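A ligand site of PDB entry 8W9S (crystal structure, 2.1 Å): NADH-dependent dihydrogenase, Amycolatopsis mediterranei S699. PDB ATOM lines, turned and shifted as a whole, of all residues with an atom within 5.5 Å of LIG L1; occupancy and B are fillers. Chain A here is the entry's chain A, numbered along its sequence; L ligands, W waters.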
ATOM      1  N   ILE A  24      -3.223  14.482  17.364  1.00  0.00           N
ATOM      2  CA  ILE A  24      -2.165  14.129  16.418  1.00  0.00           C
ATOM      3  C   ILE A  24      -2.765  13.285  15.301  1.00  0.00           C
ATOM      4  O   ILE A  24      -3.446  12.273  15.559  1.00  0.00           O
ATOM      5  CB  ILE A  24      -1.013  13.380  17.119  1.00  0.00           C
ATOM      6  CG1 ILE A  24      -0.617  14.104  18.405  1.00  0.00           C
ATOM      7  CG2 ILE A  24       0.194  13.282  16.192  1.00  0.00           C
ATOM      8  CD1 ILE A  24      -0.307  15.605  18.227  1.00  0.00           C
ATOM      9  N   GLY A  25      -2.512  13.690  14.055  1.00  0.00           N
ATOM     10  CA  GLY A  25      -3.118  13.102  12.887  1.00  0.00           C
ATOM     11  C   GLY A  25      -4.236  13.982  12.327  1.00  0.00           C
ATOM     12  O   GLY A  25      -4.845  14.793  13.034  1.00  0.00           O
ATOM     13  N   ALA A  26      -4.499  13.816  11.037  1.00  0.00           N
ATOM     14  CA  ALA A  26      -5.550  14.597  10.375  1.00  0.00           C
ATOM     15  C   ALA A  26      -6.366  13.739   9.421  1.00  0.00           C
ATOM     16  O   ALA A  26      -6.921  14.245   8.440  1.00  0.00           O
ATOM     17  CB  ALA A  26      -4.966  15.808   9.635  1.00  0.00           C
ATOM     18  N   GLY A  27      -6.446  12.437   9.690  1.00  0.00           N
ATOM     19  CA  GLY A  27      -7.210  11.524   8.872  1.00  0.00           C
ATOM     20  C   GLY A  27      -8.662  11.439   9.303  1.00  0.00           C
ATOM     21  O   GLY A  27      -9.206  12.331   9.955  1.00  0.00           O
ATOM     22  N   LEU A  28      -9.299  10.330   8.931  1.00  0.00           N
ATOM     23  CA  LEU A  28     -10.738  10.181   9.176  1.00  0.00           C
ATOM     24  C   LEU A  28     -11.058  10.068  10.657  1.00  0.00           C
ATOM     25  O   LEU A  28     -12.013  10.690  11.140  1.00  0.00           O
ATOM     26  CB  LEU A  28     -11.281   8.996   8.382  1.00  0.00           C
ATOM     27  CG  LEU A  28     -12.756   8.668   8.596  1.00  0.00           C
ATOM     28  CD1 LEU A  28     -13.639   9.879   8.332  1.00  0.00           C
ATOM     29  CD2 LEU A  28     -13.102   7.574   7.586  1.00  0.00           C
ATOM     30  N   ILE A  29     -10.257   9.311  11.419  1.00  0.00           N
ATOM     31  CA  ILE A  29     -10.498   9.181  12.857  1.00  0.00           C
ATOM     32  C   ILE A  29     -10.270  10.513  13.555  1.00  0.00           C
ATOM     33  O   ILE A  29     -11.102  10.949  14.361  1.00  0.00           O
ATOM     34  CB  ILE A  29      -9.622   8.066  13.461  1.00  0.00           C
ATOM     35  CG1 ILE A  29     -10.072   6.718  12.966  1.00  0.00           C
ATOM     36  CG2 ILE A  29      -9.762   8.020  14.991  1.00  0.00           C
ATOM     37  CD1 ILE A  29     -11.469   6.370  13.438  1.00  0.00           C
ATOM     38  N   ALA A  30      -9.140  11.164  13.271  1.00  0.00           N
ATOM     39  CA  ALA A  30      -8.847  12.472  13.833  1.00  0.00           C
ATOM     40  C   ALA A  30      -9.999  13.437  13.601  1.00  0.00           C
ATOM     41  O   ALA A  30     -10.405  14.175  14.504  1.00  0.00           O
ATOM     42  CB  ALA A  30      -7.558  13.039  13.242  1.00  0.00           C
ATOM     43  N   TYR A  47      -1.952  18.635  15.108  1.00  0.00           N
ATOM     44  CA  TYR A  47      -0.712  18.469  14.380  1.00  0.00           C
ATOM     45  C   TYR A  47      -0.716  17.153  13.623  1.00  0.00           C
ATOM     46  O   TYR A  47      -0.945  16.089  14.223  1.00  0.00           O
ATOM     47  CB  TYR A  47       0.518  18.496  15.290  1.00  0.00           C
ATOM     48  CG  TYR A  47       1.746  18.054  14.540  1.00  0.00           C
ATOM     49  CD1 TYR A  47       2.296  18.840  13.527  1.00  0.00           C
ATOM     50  CD2 TYR A  47       2.338  16.813  14.799  1.00  0.00           C
ATOM     51  CE1 TYR A  47       3.411  18.426  12.815  1.00  0.00           C
ATOM     52  CE2 TYR A  47       3.444  16.386  14.093  1.00  0.00           C
ATOM     53  CZ  TYR A  47       3.982  17.197  13.104  1.00  0.00           C
ATOM     54  OH  TYR A  47       5.093  16.772  12.411  1.00  0.00           O
ATOM     55  N   SER A  48      -0.433  17.215  12.327  1.00  0.00           N
ATOM     56  CA  SER A  48      -0.137  16.024  11.539  1.00  0.00           C
ATOM     57  C   SER A  48       1.086  16.287  10.674  1.00  0.00           C
ATOM     58  O   SER A  48       1.327  17.421  10.242  1.00  0.00           O
ATOM     59  CB  SER A  48      -1.327  15.610  10.659  1.00  0.00           C
ATOM     60  OG  SER A  48      -1.605  16.612   9.691  1.00  0.00           O
ATOM     61  N   ASP A  49       1.861  15.235  10.430  1.00  0.00           N
ATOM     62  CA  ASP A  49       3.083  15.368   9.649  1.00  0.00           C
ATOM     63  C   ASP A  49       2.823  15.565   8.162  1.00  0.00           C
ATOM     64  O   ASP A  49       3.769  15.811   7.414  1.00  0.00           O
ATOM     65  CB  ASP A  49       4.015  14.165   9.900  1.00  0.00           C
ATOM     66  CG  ASP A  49       3.526  12.847   9.247  1.00  0.00           C
ATOM     67  OD1 ASP A  49       4.293  11.858   9.317  1.00  0.00           O
ATOM     68  OD2 ASP A  49       2.401  12.789   8.694  1.00  0.00           O
ATOM     69  N   ASP A  50       1.569  15.467   7.719  1.00  0.00           N
ATOM     70  CA  ASP A  50       1.255  15.711   6.315  1.00  0.00           C
ATOM     71  C   ASP A  50       0.848  17.147   6.057  1.00  0.00           C
ATOM     72  O   ASP A  50       0.480  17.481   4.926  1.00  0.00           O
ATOM     73  CB  ASP A  50       0.145  14.759   5.822  1.00  0.00           C
ATOM     74  CG  ASP A  50      -1.191  14.949   6.551  1.00  0.00           C
ATOM     75  OD1 ASP A  50      -1.304  15.834   7.429  1.00  0.00           O
ATOM     76  OD2 ASP A  50      -2.132  14.200   6.241  1.00  0.00           O
ATOM     77  N   ARG A  52      -1.824  18.531   6.654  1.00  0.00           N
ATOM     78  CA  ARG A  52      -3.273  18.653   6.532  1.00  0.00           C
ATOM     79  C   ARG A  52      -3.948  19.088   7.831  1.00  0.00           C
ATOM     80  O   ARG A  52      -5.141  19.404   7.814  1.00  0.00           O
ATOM     81  CB  ARG A  52      -3.873  17.334   6.038  1.00  0.00           C
ATOM     82  CG  ARG A  52      -4.014  17.208   4.508  1.00  0.00           C
ATOM     83  CD  ARG A  52      -2.725  17.582   3.782  1.00  0.00           C
ATOM     84  NE  ARG A  52      -2.861  17.546   2.319  1.00  0.00           N
ATOM     85  CZ  ARG A  52      -1.861  17.277   1.472  1.00  0.00           C
ATOM     86  NH1 ARG A  52      -0.647  17.017   1.932  1.00  0.00           N
ATOM     87  NH2 ARG A  52      -2.076  17.283   0.163  1.00  0.00           N
ATOM     88  N   CYS A  81      -4.163   9.823  16.847  1.00  0.00           N
ATOM     89  CA  CYS A  81      -4.989   9.335  15.746  1.00  0.00           C
ATOM     90  C   CYS A  81      -4.130   9.148  14.502  1.00  0.00           C
ATOM     91  O   CYS A  81      -4.536   9.482  13.385  1.00  0.00           O
ATOM     92  CB  CYS A  81      -6.144  10.288  15.479  1.00  0.00           C
ATOM     93  SG  CYS A  81      -7.407  10.275  16.762  1.00  0.00           S
ATOM     94  N   THR A  82      -2.942   8.610  14.706  1.00  0.00           N
ATOM     95  CA  THR A  82      -1.958   8.305  13.680  1.00  0.00           C
ATOM     96  C   THR A  82      -1.916   6.807  13.437  1.00  0.00           C
ATOM     97  O   THR A  82      -2.464   6.011  14.204  1.00  0.00           O
ATOM     98  CB  THR A  82      -0.571   8.797  14.124  1.00  0.00           C
ATOM     99  OG1 THR A  82      -0.194   8.133  15.340  1.00  0.00           O
ATOM    100  CG2 THR A  82      -0.559  10.317  14.311  1.00  0.00           C
ATOM    101  N   PRO A  83      -1.256   6.369  12.352  1.00  0.00           N
ATOM    102  CA  PRO A  83      -1.062   4.933  12.139  1.00  0.00           C
ATOM    103  C   PRO A  83      -0.442   4.259  13.348  1.00  0.00           C
ATOM    104  O   PRO A  83       0.386   4.830  14.064  1.00  0.00           O
ATOM    105  CB  PRO A  83      -0.112   4.879  10.935  1.00  0.00           C
ATOM    106  CG  PRO A  83      -0.324   6.166  10.213  1.00  0.00           C
ATOM    107  CD  PRO A  83      -0.828   7.176  11.190  1.00  0.00           C
ATOM    108  N   THR A  84      -0.827   2.991  13.521  1.00  0.00           N
ATOM    109  CA  THR A  84      -0.466   2.220  14.701  1.00  0.00           C
ATOM    110  C   THR A  84       1.029   2.206  14.993  1.00  0.00           C
ATOM    111  O   THR A  84       1.435   2.373  16.152  1.00  0.00           O
ATOM    112  CB  THR A  84      -0.986   0.790  14.525  1.00  0.00           C
ATOM    113  OG1 THR A  84      -2.403   0.846  14.380  1.00  0.00           O
ATOM    114  CG2 THR A  84      -0.609  -0.056  15.720  1.00  0.00           C
ATOM    115  N   SER A  86       3.245   4.289  14.712  1.00  0.00           N
ATOM    116  CA  SER A  86       3.752   5.516  15.329  1.00  0.00           C
ATOM    117  C   SER A  86       3.197   5.771  16.720  1.00  0.00           C
ATOM    118  O   SER A  86       3.588   6.763  17.346  1.00  0.00           O
ATOM    119  CB  SER A  86       3.446   6.705  14.422  1.00  0.00           C
ATOM    120  OG  SER A  86       2.078   7.050  14.506  1.00  0.00           O
ATOM    121  N   HIS A  87       2.314   4.903  17.231  1.00  0.00           N
ATOM    122  CA  HIS A  87       1.720   5.144  18.548  1.00  0.00           C
ATOM    123  C   HIS A  87       2.774   5.119  19.643  1.00  0.00           C
ATOM    124  O   HIS A  87       2.724   5.937  20.578  1.00  0.00           O
ATOM    125  CB  HIS A  87       0.637   4.111  18.850  1.00  0.00           C
ATOM    126  CG  HIS A  87      -0.581   4.230  17.994  1.00  0.00           C
ATOM    127  ND1 HIS A  87      -1.684   3.400  18.130  1.00  0.00           N
ATOM    128  CD2 HIS A  87      -0.879   5.073  16.977  1.00  0.00           C
ATOM    129  CE1 HIS A  87      -2.591   3.729  17.240  1.00  0.00           C
ATOM    130  NE2 HIS A  87      -2.139   4.737  16.525  1.00  0.00           N
ATOM    131  N   ILE A  90       5.018   8.452  19.875  1.00  0.00           N
ATOM    132  CA  ILE A  90       4.195   9.620  20.187  1.00  0.00           C
ATOM    133  C   ILE A  90       3.691   9.542  21.633  1.00  0.00           C
ATOM    134  O   ILE A  90       3.789  10.512  22.392  1.00  0.00           O
ATOM    135  CB  ILE A  90       3.040   9.756  19.188  1.00  0.00           C
ATOM    136  CG1 ILE A  90       3.594   9.964  17.784  1.00  0.00           C
ATOM    137  CG2 ILE A  90       2.129  10.909  19.575  1.00  0.00           C
ATOM    138  CD1 ILE A  90       2.544  10.138  16.723  1.00  0.00           C
ATOM    139  N   GLU A 104      -5.741   5.831  19.777  1.00  0.00           N
ATOM    140  CA  GLU A 104      -6.604   4.981  18.978  1.00  0.00           C
ATOM    141  C   GLU A 104      -6.133   3.524  19.039  1.00  0.00           C
ATOM    142  O   GLU A 104      -4.954   3.240  19.270  1.00  0.00           O
ATOM    143  CB  GLU A 104      -6.643   5.508  17.556  1.00  0.00           C
ATOM    144  CG  GLU A 104      -7.435   4.702  16.606  1.00  0.00           C
ATOM    145  CD  GLU A 104      -8.930   4.684  16.842  1.00  0.00           C
ATOM    146  OE1 GLU A 104      -9.647   4.264  15.910  1.00  0.00           O
ATOM    147  OE2 GLU A 104      -9.406   5.082  17.932  1.00  0.00           O
ATOM    148  N   LYS A 105      -7.083   2.604  18.877  1.00  0.00           N
ATOM    149  CA  LYS A 105      -6.800   1.175  18.952  1.00  0.00           C
ATOM    150  C   LYS A 105      -6.107   0.695  17.677  1.00  0.00           C
ATOM    151  O   LYS A 105      -6.337   1.244  16.593  1.00  0.00           O
ATOM    152  CB  LYS A 105      -8.112   0.417  19.155  1.00  0.00           C
ATOM    153  CG  LYS A 105      -9.062   0.558  17.992  1.00  0.00           C
ATOM    154  CD  LYS A 105     -10.465   0.078  18.313  1.00  0.00           C
ATOM    155  CE  LYS A 105     -11.474   0.812  17.428  1.00  0.00           C
ATOM    156  NZ  LYS A 105     -11.208   2.295  17.386  1.00  0.00           N
ATOM    157  N   PRO A 106      -5.224  -0.314  17.767  1.00  0.00           N
ATOM    158  CA  PRO A 106      -4.722  -0.925  19.003  1.00  0.00           C
ATOM    159  C   PRO A 106      -3.681  -0.015  19.623  1.00  0.00           C
ATOM    160  O   PRO A 106      -3.090   0.773  18.885  1.00  0.00           O
ATOM    161  CB  PRO A 106      -4.091  -2.243  18.531  1.00  0.00           C
ATOM    162  CG  PRO A 106      -3.828  -2.083  17.095  1.00  0.00           C
ATOM    163  CD  PRO A 106      -4.633  -0.925  16.563  1.00  0.00           C
ATOM    164  N   ASP A 133     -13.943   1.805  20.898  1.00  0.00           N
ATOM    165  CA  ASP A 133     -15.242   2.443  20.681  1.00  0.00           C
ATOM    166  C   ASP A 133     -16.419   1.544  21.042  1.00  0.00           C
ATOM    167  O   ASP A 133     -17.473   2.040  21.439  1.00  0.00           O
ATOM    168  CB  ASP A 133     -15.395   2.879  19.218  1.00  0.00           C
ATOM    169  CG  ASP A 133     -14.181   3.616  18.679  1.00  0.00           C
ATOM    170  OD1 ASP A 133     -13.656   3.177  17.632  1.00  0.00           O
ATOM    171  OD2 ASP A 133     -13.737   4.614  19.276  1.00  0.00           O
ATOM    172  N   ARG A 168     -12.501   1.874   2.361  1.00  0.00           N
ATOM    173  CA  ARG A 168     -11.264   2.520   1.967  1.00  0.00           C
ATOM    174  C   ARG A 168     -10.210   1.441   1.781  1.00  0.00           C
ATOM    175  O   ARG A 168     -10.333   0.338   2.324  1.00  0.00           O
ATOM    176  CB  ARG A 168     -10.755   3.503   3.041  1.00  0.00           C
ATOM    177  CG  ARG A 168     -11.821   4.262   3.788  1.00  0.00           C
ATOM    178  CD  ARG A 168     -11.221   5.330   4.735  1.00  0.00           C
ATOM    179  NE  ARG A 168     -10.842   4.780   6.038  1.00  0.00           N
ATOM    180  CZ  ARG A 168      -9.873   5.260   6.815  1.00  0.00           C
ATOM    181  NH1 ARG A 168      -9.158   6.316   6.421  1.00  0.00           N
ATOM    182  NH2 ARG A 168      -9.616   4.699   7.998  1.00  0.00           N
ATOM    183  N   ASP A 184      -7.388  -5.969  12.543  1.00  0.00           N
ATOM    184  CA  ASP A 184      -8.209  -4.754  12.692  1.00  0.00           C
ATOM    185  C   ASP A 184      -9.618  -5.083  13.158  1.00  0.00           C
ATOM    186  O   ASP A 184     -10.174  -4.368  14.007  1.00  0.00           O
ATOM    187  CB  ASP A 184      -8.284  -3.999  11.366  1.00  0.00           C
ATOM    188  CG  ASP A 184      -6.950  -3.428  10.918  1.00  0.00           C
ATOM    189  OD1 ASP A 184      -6.116  -3.090  11.795  1.00  0.00           O
ATOM    190  OD2 ASP A 184      -6.755  -3.309   9.699  1.00  0.00           O
ATOM    191  N   LEU A 187     -10.110  -6.667  17.010  1.00  0.00           N
ATOM    192  CA  LEU A 187      -9.955  -5.925  18.255  1.00  0.00           C
ATOM    193  C   LEU A 187     -11.305  -5.625  18.917  1.00  0.00           C
ATOM    194  O   LEU A 187     -11.400  -5.630  20.146  1.00  0.00           O
ATOM    195  CB  LEU A 187      -9.131  -4.665  18.028  1.00  0.00           C
ATOM    196  CG  LEU A 187      -8.711  -4.065  19.381  1.00  0.00           C
ATOM    197  CD1 LEU A 187      -7.343  -3.465  19.245  1.00  0.00           C
ATOM    198  CD2 LEU A 187      -9.700  -2.980  19.902  1.00  0.00           C
ATOM    199  N   HIS A 188     -12.375  -5.400  18.138  1.00  0.00           N
ATOM    200  CA  HIS A 188     -13.683  -5.172  18.743  1.00  0.00           C
ATOM    201  C   HIS A 188     -14.120  -6.385  19.557  1.00  0.00           C
ATOM    202  O   HIS A 188     -14.458  -6.281  20.737  1.00  0.00           O
ATOM    203  CB  HIS A 188     -14.753  -4.870  17.682  1.00  0.00           C
ATOM    204  CG  HIS A 188     -14.388  -3.755  16.767  1.00  0.00           C
ATOM    205  ND1 HIS A 188     -14.164  -2.471  17.206  1.00  0.00           N
ATOM    206  CD2 HIS A 188     -14.208  -3.735  15.425  1.00  0.00           C
ATOM    207  CE1 HIS A 188     -13.869  -1.701  16.172  1.00  0.00           C
ATOM    208  NE2 HIS A 188     -13.879  -2.446  15.078  1.00  0.00           N
HETATM  209  P1  LIG L   1      -5.260   7.747   8.240  1.00  0.00           P
HETATM  210  O1  LIG L   1      -4.227   7.288   7.260  1.00  0.00           O
HETATM  211  O2  LIG L   1      -6.505   8.314   7.553  1.00  0.00           O
HETATM  212  O3  LIG L   1      -4.609   8.918   9.233  1.00  0.00           O
HETATM  213  C1  LIG L   1      -3.204   9.050   9.342  1.00  0.00           C
HETATM  214  C2  LIG L   1      -2.942  10.539   9.792  1.00  0.00           C
HETATM  215  O4  LIG L   1      -1.964  10.575  10.660  1.00  0.00           O
HETATM  216  C3  LIG L   1      -2.459  11.367   8.521  1.00  0.00           C
HETATM  217  O5  LIG L   1      -3.020  12.676   8.591  1.00  0.00           O
HETATM  218  C4  LIG L   1      -0.936  11.360   8.663  1.00  0.00           C
HETATM  219  O6  LIG L   1      -0.375  12.496   8.006  1.00  0.00           O
HETATM  220  C5  LIG L   1      -0.746  11.435   9.990  1.00  0.00           C
HETATM  221  N1  LIG L   1       0.499  10.907  10.562  1.00  0.00           N
HETATM  222  C6  LIG L   1       1.100   9.761  10.232  1.00  0.00           C
HETATM  223  N2  LIG L   1       2.190   9.621  10.950  1.00  0.00           N
HETATM  224  C7  LIG L   1       2.314  10.689  11.773  1.00  0.00           C
HETATM  225  C8  LIG L   1       3.232  11.119  12.756  1.00  0.00           C
HETATM  226  N3  LIG L   1       4.368  10.318  13.080  1.00  0.00           N
HETATM  227  N4  LIG L   1       3.044  12.273  13.408  1.00  0.00           N
HETATM  228  C9  LIG L   1       1.998  13.013  13.121  1.00  0.00           C
HETATM  229  N5  LIG L   1       1.104  12.658  12.201  1.00  0.00           N
HETATM  230  C10 LIG L   1       1.227  11.503  11.520  1.00  0.00           C
HETATM  231  O7  LIG L   1      -5.679   6.459   9.160  1.00  0.00           O
HETATM  232  P2  LIG L   1      -6.847   6.528  10.299  1.00  0.00           P
HETATM  233  O8  LIG L   1      -7.561   7.847  10.304  1.00  0.00           O
HETATM  234  O9  LIG L   1      -7.830   5.419  10.084  1.00  0.00           O
HETATM  235  O10 LIG L   1      -6.012   6.288  11.694  1.00  0.00           O
HETATM  236  C11 LIG L   1      -5.194   5.142  11.703  1.00  0.00           C
HETATM  237  C12 LIG L   1      -5.202   4.680  13.194  1.00  0.00           C
HETATM  238  O11 LIG L   1      -6.432   4.682  13.647  1.00  0.00           O
HETATM  239  C13 LIG L   1      -4.670   3.147  13.252  1.00  0.00           C
HETATM  240  O12 LIG L   1      -4.198   2.960  14.508  1.00  0.00           O
HETATM  241  C14 LIG L   1      -5.722   2.435  12.986  1.00  0.00           C
HETATM  242  O13 LIG L   1      -5.635   1.132  13.467  1.00  0.00           O
HETATM  243  C15 LIG L   1      -6.826   3.195  13.801  1.00  0.00           C
HETATM  244  N6  LIG L   1      -8.225   2.847  13.405  1.00  0.00           N
HETATM  245  C16 LIG L   1      -8.780   1.758  13.912  1.00  0.00           C
HETATM  246  C17 LIG L   1     -10.072   1.381  13.572  1.00  0.00           C
HETATM  247  C18 LIG L   1     -10.737   0.085  14.159  1.00  0.00           C
HETATM  248  O14 LIG L   1     -10.083  -0.868  14.405  1.00  0.00           O
HETATM  249  N7  LIG L   1     -12.203   0.089  14.388  1.00  0.00           N
HETATM  250  C19 LIG L   1     -10.796   2.203  12.701  1.00  0.00           C
HETATM  251  C20 LIG L   1     -10.192   3.335  12.182  1.00  0.00           C
HETATM  252  C21 LIG L   1      -8.883   3.628  12.569  1.00  0.00           C
HETATM  253  C1  LG2 L   2     -20.016   0.552  17.906  1.00  0.00           C
HETATM  254  C2  LG2 L   2     -19.274   0.575  16.578  1.00  0.00           C
HETATM  255  C3  LG2 L   2     -19.351  -0.827  15.941  1.00  0.00           C
HETATM  256  C4  LG2 L   2     -18.365  -1.279  15.117  1.00  0.00           C
HETATM  257  C5  LG2 L   2     -18.509  -2.706  14.472  1.00  0.00           C
HETATM  258  C6  LG2 L   2     -17.930  -3.042  13.286  1.00  0.00           C
HETATM  259  C7  LG2 L   2     -17.043  -2.045  12.504  1.00  0.00           C
HETATM  260  C8  LG2 L   2     -14.987  -1.695  11.101  1.00  0.00           C
HETATM  261  C9  LG2 L   2     -15.542  -0.758  10.082  1.00  0.00           C
HETATM  262  C10 LG2 L   2     -14.596   0.170   9.344  1.00  0.00           C
HETATM  263  C11 LG2 L   2     -13.062   0.147   9.654  1.00  0.00           C
HETATM  264  C12 LG2 L   2     -12.142   1.002   8.961  1.00  0.00           C
HETATM  265  C13 LG2 L   2     -10.765   0.965   9.281  1.00  0.00           C
HETATM  266  C14 LG2 L   2     -10.253   0.053  10.243  1.00  0.00           C
HETATM  267  C15 LG2 L   2     -11.152  -0.809  10.935  1.00  0.00           C
HETATM  268  C16 LG2 L   2     -12.564  -0.763  10.636  1.00  0.00           C
HETATM  269  C17 LG2 L   2     -13.526  -1.728  11.417  1.00  0.00           C
HETATM  270  C18 LG2 L   2      -8.734   0.041  10.541  1.00  0.00           C
HETATM  271  C19 LG2 L   2     -12.570   2.090   7.905  1.00  0.00           C
HETATM  272  C20 LG2 L   2     -13.556   3.205   8.435  1.00  0.00           C
HETATM  273  C21 LG2 L   2     -13.620   3.451   9.792  1.00  0.00           C
HETATM  274  C22 LG2 L   2     -14.560   4.519  10.413  1.00  0.00           C
HETATM  275  C23 LG2 L   2     -15.165   4.005  11.721  1.00  0.00           C
HETATM  276  C24 LG2 L   2     -16.678   3.744  11.554  1.00  0.00           C
HETATM  277  C25 LG2 L   2     -17.365   3.404  12.895  1.00  0.00           C
HETATM  278  C26 LG2 L   2     -18.859   3.803  12.818  1.00  0.00           C
HETATM  279  C27 LG2 L   2     -19.615   3.377  14.093  1.00  0.00           C
HETATM  280  C28 LG2 L   2     -19.429   1.881  14.363  1.00  0.00           C
HETATM  281  C29 LG2 L   2     -20.072   1.570  15.735  1.00  0.00           C
HETATM  282  C30 LG2 L   2     -20.132   1.102  13.282  1.00  0.00           C
HETATM  283  C31 LG2 L   2     -18.940   5.304  12.684  1.00  0.00           C
HETATM  284  C32 LG2 L   2     -16.869   2.611  10.560  1.00  0.00           C
HETATM  285  C33 LG2 L   2     -13.759   5.737  10.794  1.00  0.00           C
HETATM  286  C34 LG2 L   2     -14.439   4.017   7.458  1.00  0.00           C
HETATM  287  C35 LG2 L   2     -18.078  -4.463  12.687  1.00  0.00           C
HETATM  288  N1  LG2 L   2     -15.880  -2.599  11.837  1.00  0.00           N
HETATM  289  O1  LG2 L   2     -17.280  -0.884  12.444  1.00  0.00           O
HETATM  290  O2  LG2 L   2     -15.061   0.894   8.535  1.00  0.00           O
HETATM  291  O3  LG2 L   2     -13.129  -2.481  12.242  1.00  0.00           O
HETATM  292  O4  LG2 L   2     -10.682  -1.723  11.899  1.00  0.00           O
HETATM  293  O5  LG2 L   2      -9.887   1.818   8.590  1.00  0.00           O
HETATM  294  O6  LG2 L   2     -12.138   2.118   6.803  1.00  0.00           O
HETATM  295  O7  LG2 L   2     -21.326   1.021  15.525  1.00  0.00           O
HETATM  296  O8  LG2 L   2     -19.194   4.131  15.195  1.00  0.00           O
HETATM  297  O9  LG2 L   2     -16.817   4.158  13.909  1.00  0.00           O
HETATM  298  O10 LG2 L   2     -14.477   2.851  12.089  1.00  0.00           O
HETATM  299  O   HOH W   1      -2.311   1.843  11.256  1.00  0.00           O
HETATM  300  O   HOH W   2      -6.345  10.284  11.869  1.00  0.00           O
HETATM  301  O   HOH W   3      -7.013  -1.012  13.727  1.00  0.00           O
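The side-chain hydroxyl (OG1) of Thr 84 is in hydrogen-bond range of an oxygen (O12) of LIG L1, at 2.8 Å.
The guanidinium group (NH2) of Arg 168 is in salt-bridge range of an oxygen (O9) of LIG L1, 2.8 Å away.
N5 of LIG L1 sits at hydrogen-bond distance from N of Asp 49, 3.2 Å away.
An oxygen (O6) of LIG L1 is in hydrogen-bond range of the side-chain carboxylate of Asp 49, at 2.9 Å.
The side-chain carboxylate of Asp 50 lies within hydrogen-bond range of an oxygen (O5) of LIG L1 (2.9 Å).
A ring nitrogen (NE2) of His 188 lies close to a nitrogen (N7) of LIG L1, 3.1 Å away.
N of Ala 26 is in hydrogen-bond range of O5 of LIG L1, at 3.1 Å.
An oxygen (O13) of LIG L1 is in hydrogen-bond range of the backbone carbonyl oxygen (O) of Lys 105 (3.2 Å).
NE2 of His 87 sits close to O12 of LIG L1 (3.4 Å).
O8 of LIG L1 lies within hydrogen-bond range of N of Ile 29, 3.3 Å away.
The backbone NH (N) of Leu 28 is in hydrogen-bond range of an oxygen (O8) of LIG L1 (3.3 Å).
The guanidinium group (NH2) of Arg 168 is in hydrogen-bond range of an oxygen (O5) of LG2 L2, 3.0 Å away.
NE2 of His 188 lies within hydrogen-bond range of O3 of LG2 L2.
O of Asp 184 lies close to O4 of LG2 L2, 3.4 Å away.
An oxygen (O4) of LG2 L2 sits at hydrogen-bond distance from an oxygen (O14) of LIG L1 (2.7 Å).
OD1 of Asp 50 is in hydrogen-bond range of OG of Ser 48, at 2.4 Å.
The side-chain carboxylate of Glu 104 lies within salt-bridge range of the side-chain amino group of Lys 105.
ND1 of His 87 sits close to O of Glu 104 (3.5 Å).
O of Thr 82 is in hydrogen-bond range of NE2 of His 87 (2.7 Å).
OG1 of Thr 82 sits at hydrogen-bond distance from OG of Ser 86 (2.7 Å).
A ring nitrogen (ND1) of His 87 lies within hydrogen-bond range of the backbone carbonyl oxygen (O) of Pro 106 (3.1 Å).
N of Gly 25 is in hydrogen-bond range of O of Tyr 47.
The backbone carbonyl oxygen (O) of Ile 24 sits at hydrogen-bond distance from the backbone NH (N) of Cys 81 (2.9 Å).
The side-chain carboxylate of Glu 104 lies close to a nitrogen (N6) of LIG L1, 3.2 Å away.
Residues that only touch LIG L1: Thr 82 (3.2 Å), Pro 83 (3.4 Å), Asp 184 (3.5 Å), Gly 27 (3.5 Å), Gly 25 (3.6 Å), Ile 24 (3.6 Å), Ser 48 (3.6 Å), Tyr 47 (3.8 Å), Pro 106 (3.8 Å), Cys 81 (3.9 Å), Ser 86 (3.96 Å) and Ile 90 (3.97 Å).
Hydrophobic or aromatic side chains within 4 Å of LIG L1: Ile 24, Ala 26, Ile 29, Tyr 47, Pro 83, His 87, Ile 90, Pro 106 and His 188.
Along chain A the residues within 4 Å of LIG L1 span positions 24 to 188.
The nearest printed residue that does not touch LIG L1 is Asp 133 (4.7 Å).
Water W3 lies within hydrogen-bond range of O13 of LIG L1 and OD1 of Asp 184.
Water W2 lies within hydrogen-bond range of O of Cys 81, N of Gly 27, O8 of LIG L1 and N of Ala 30.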
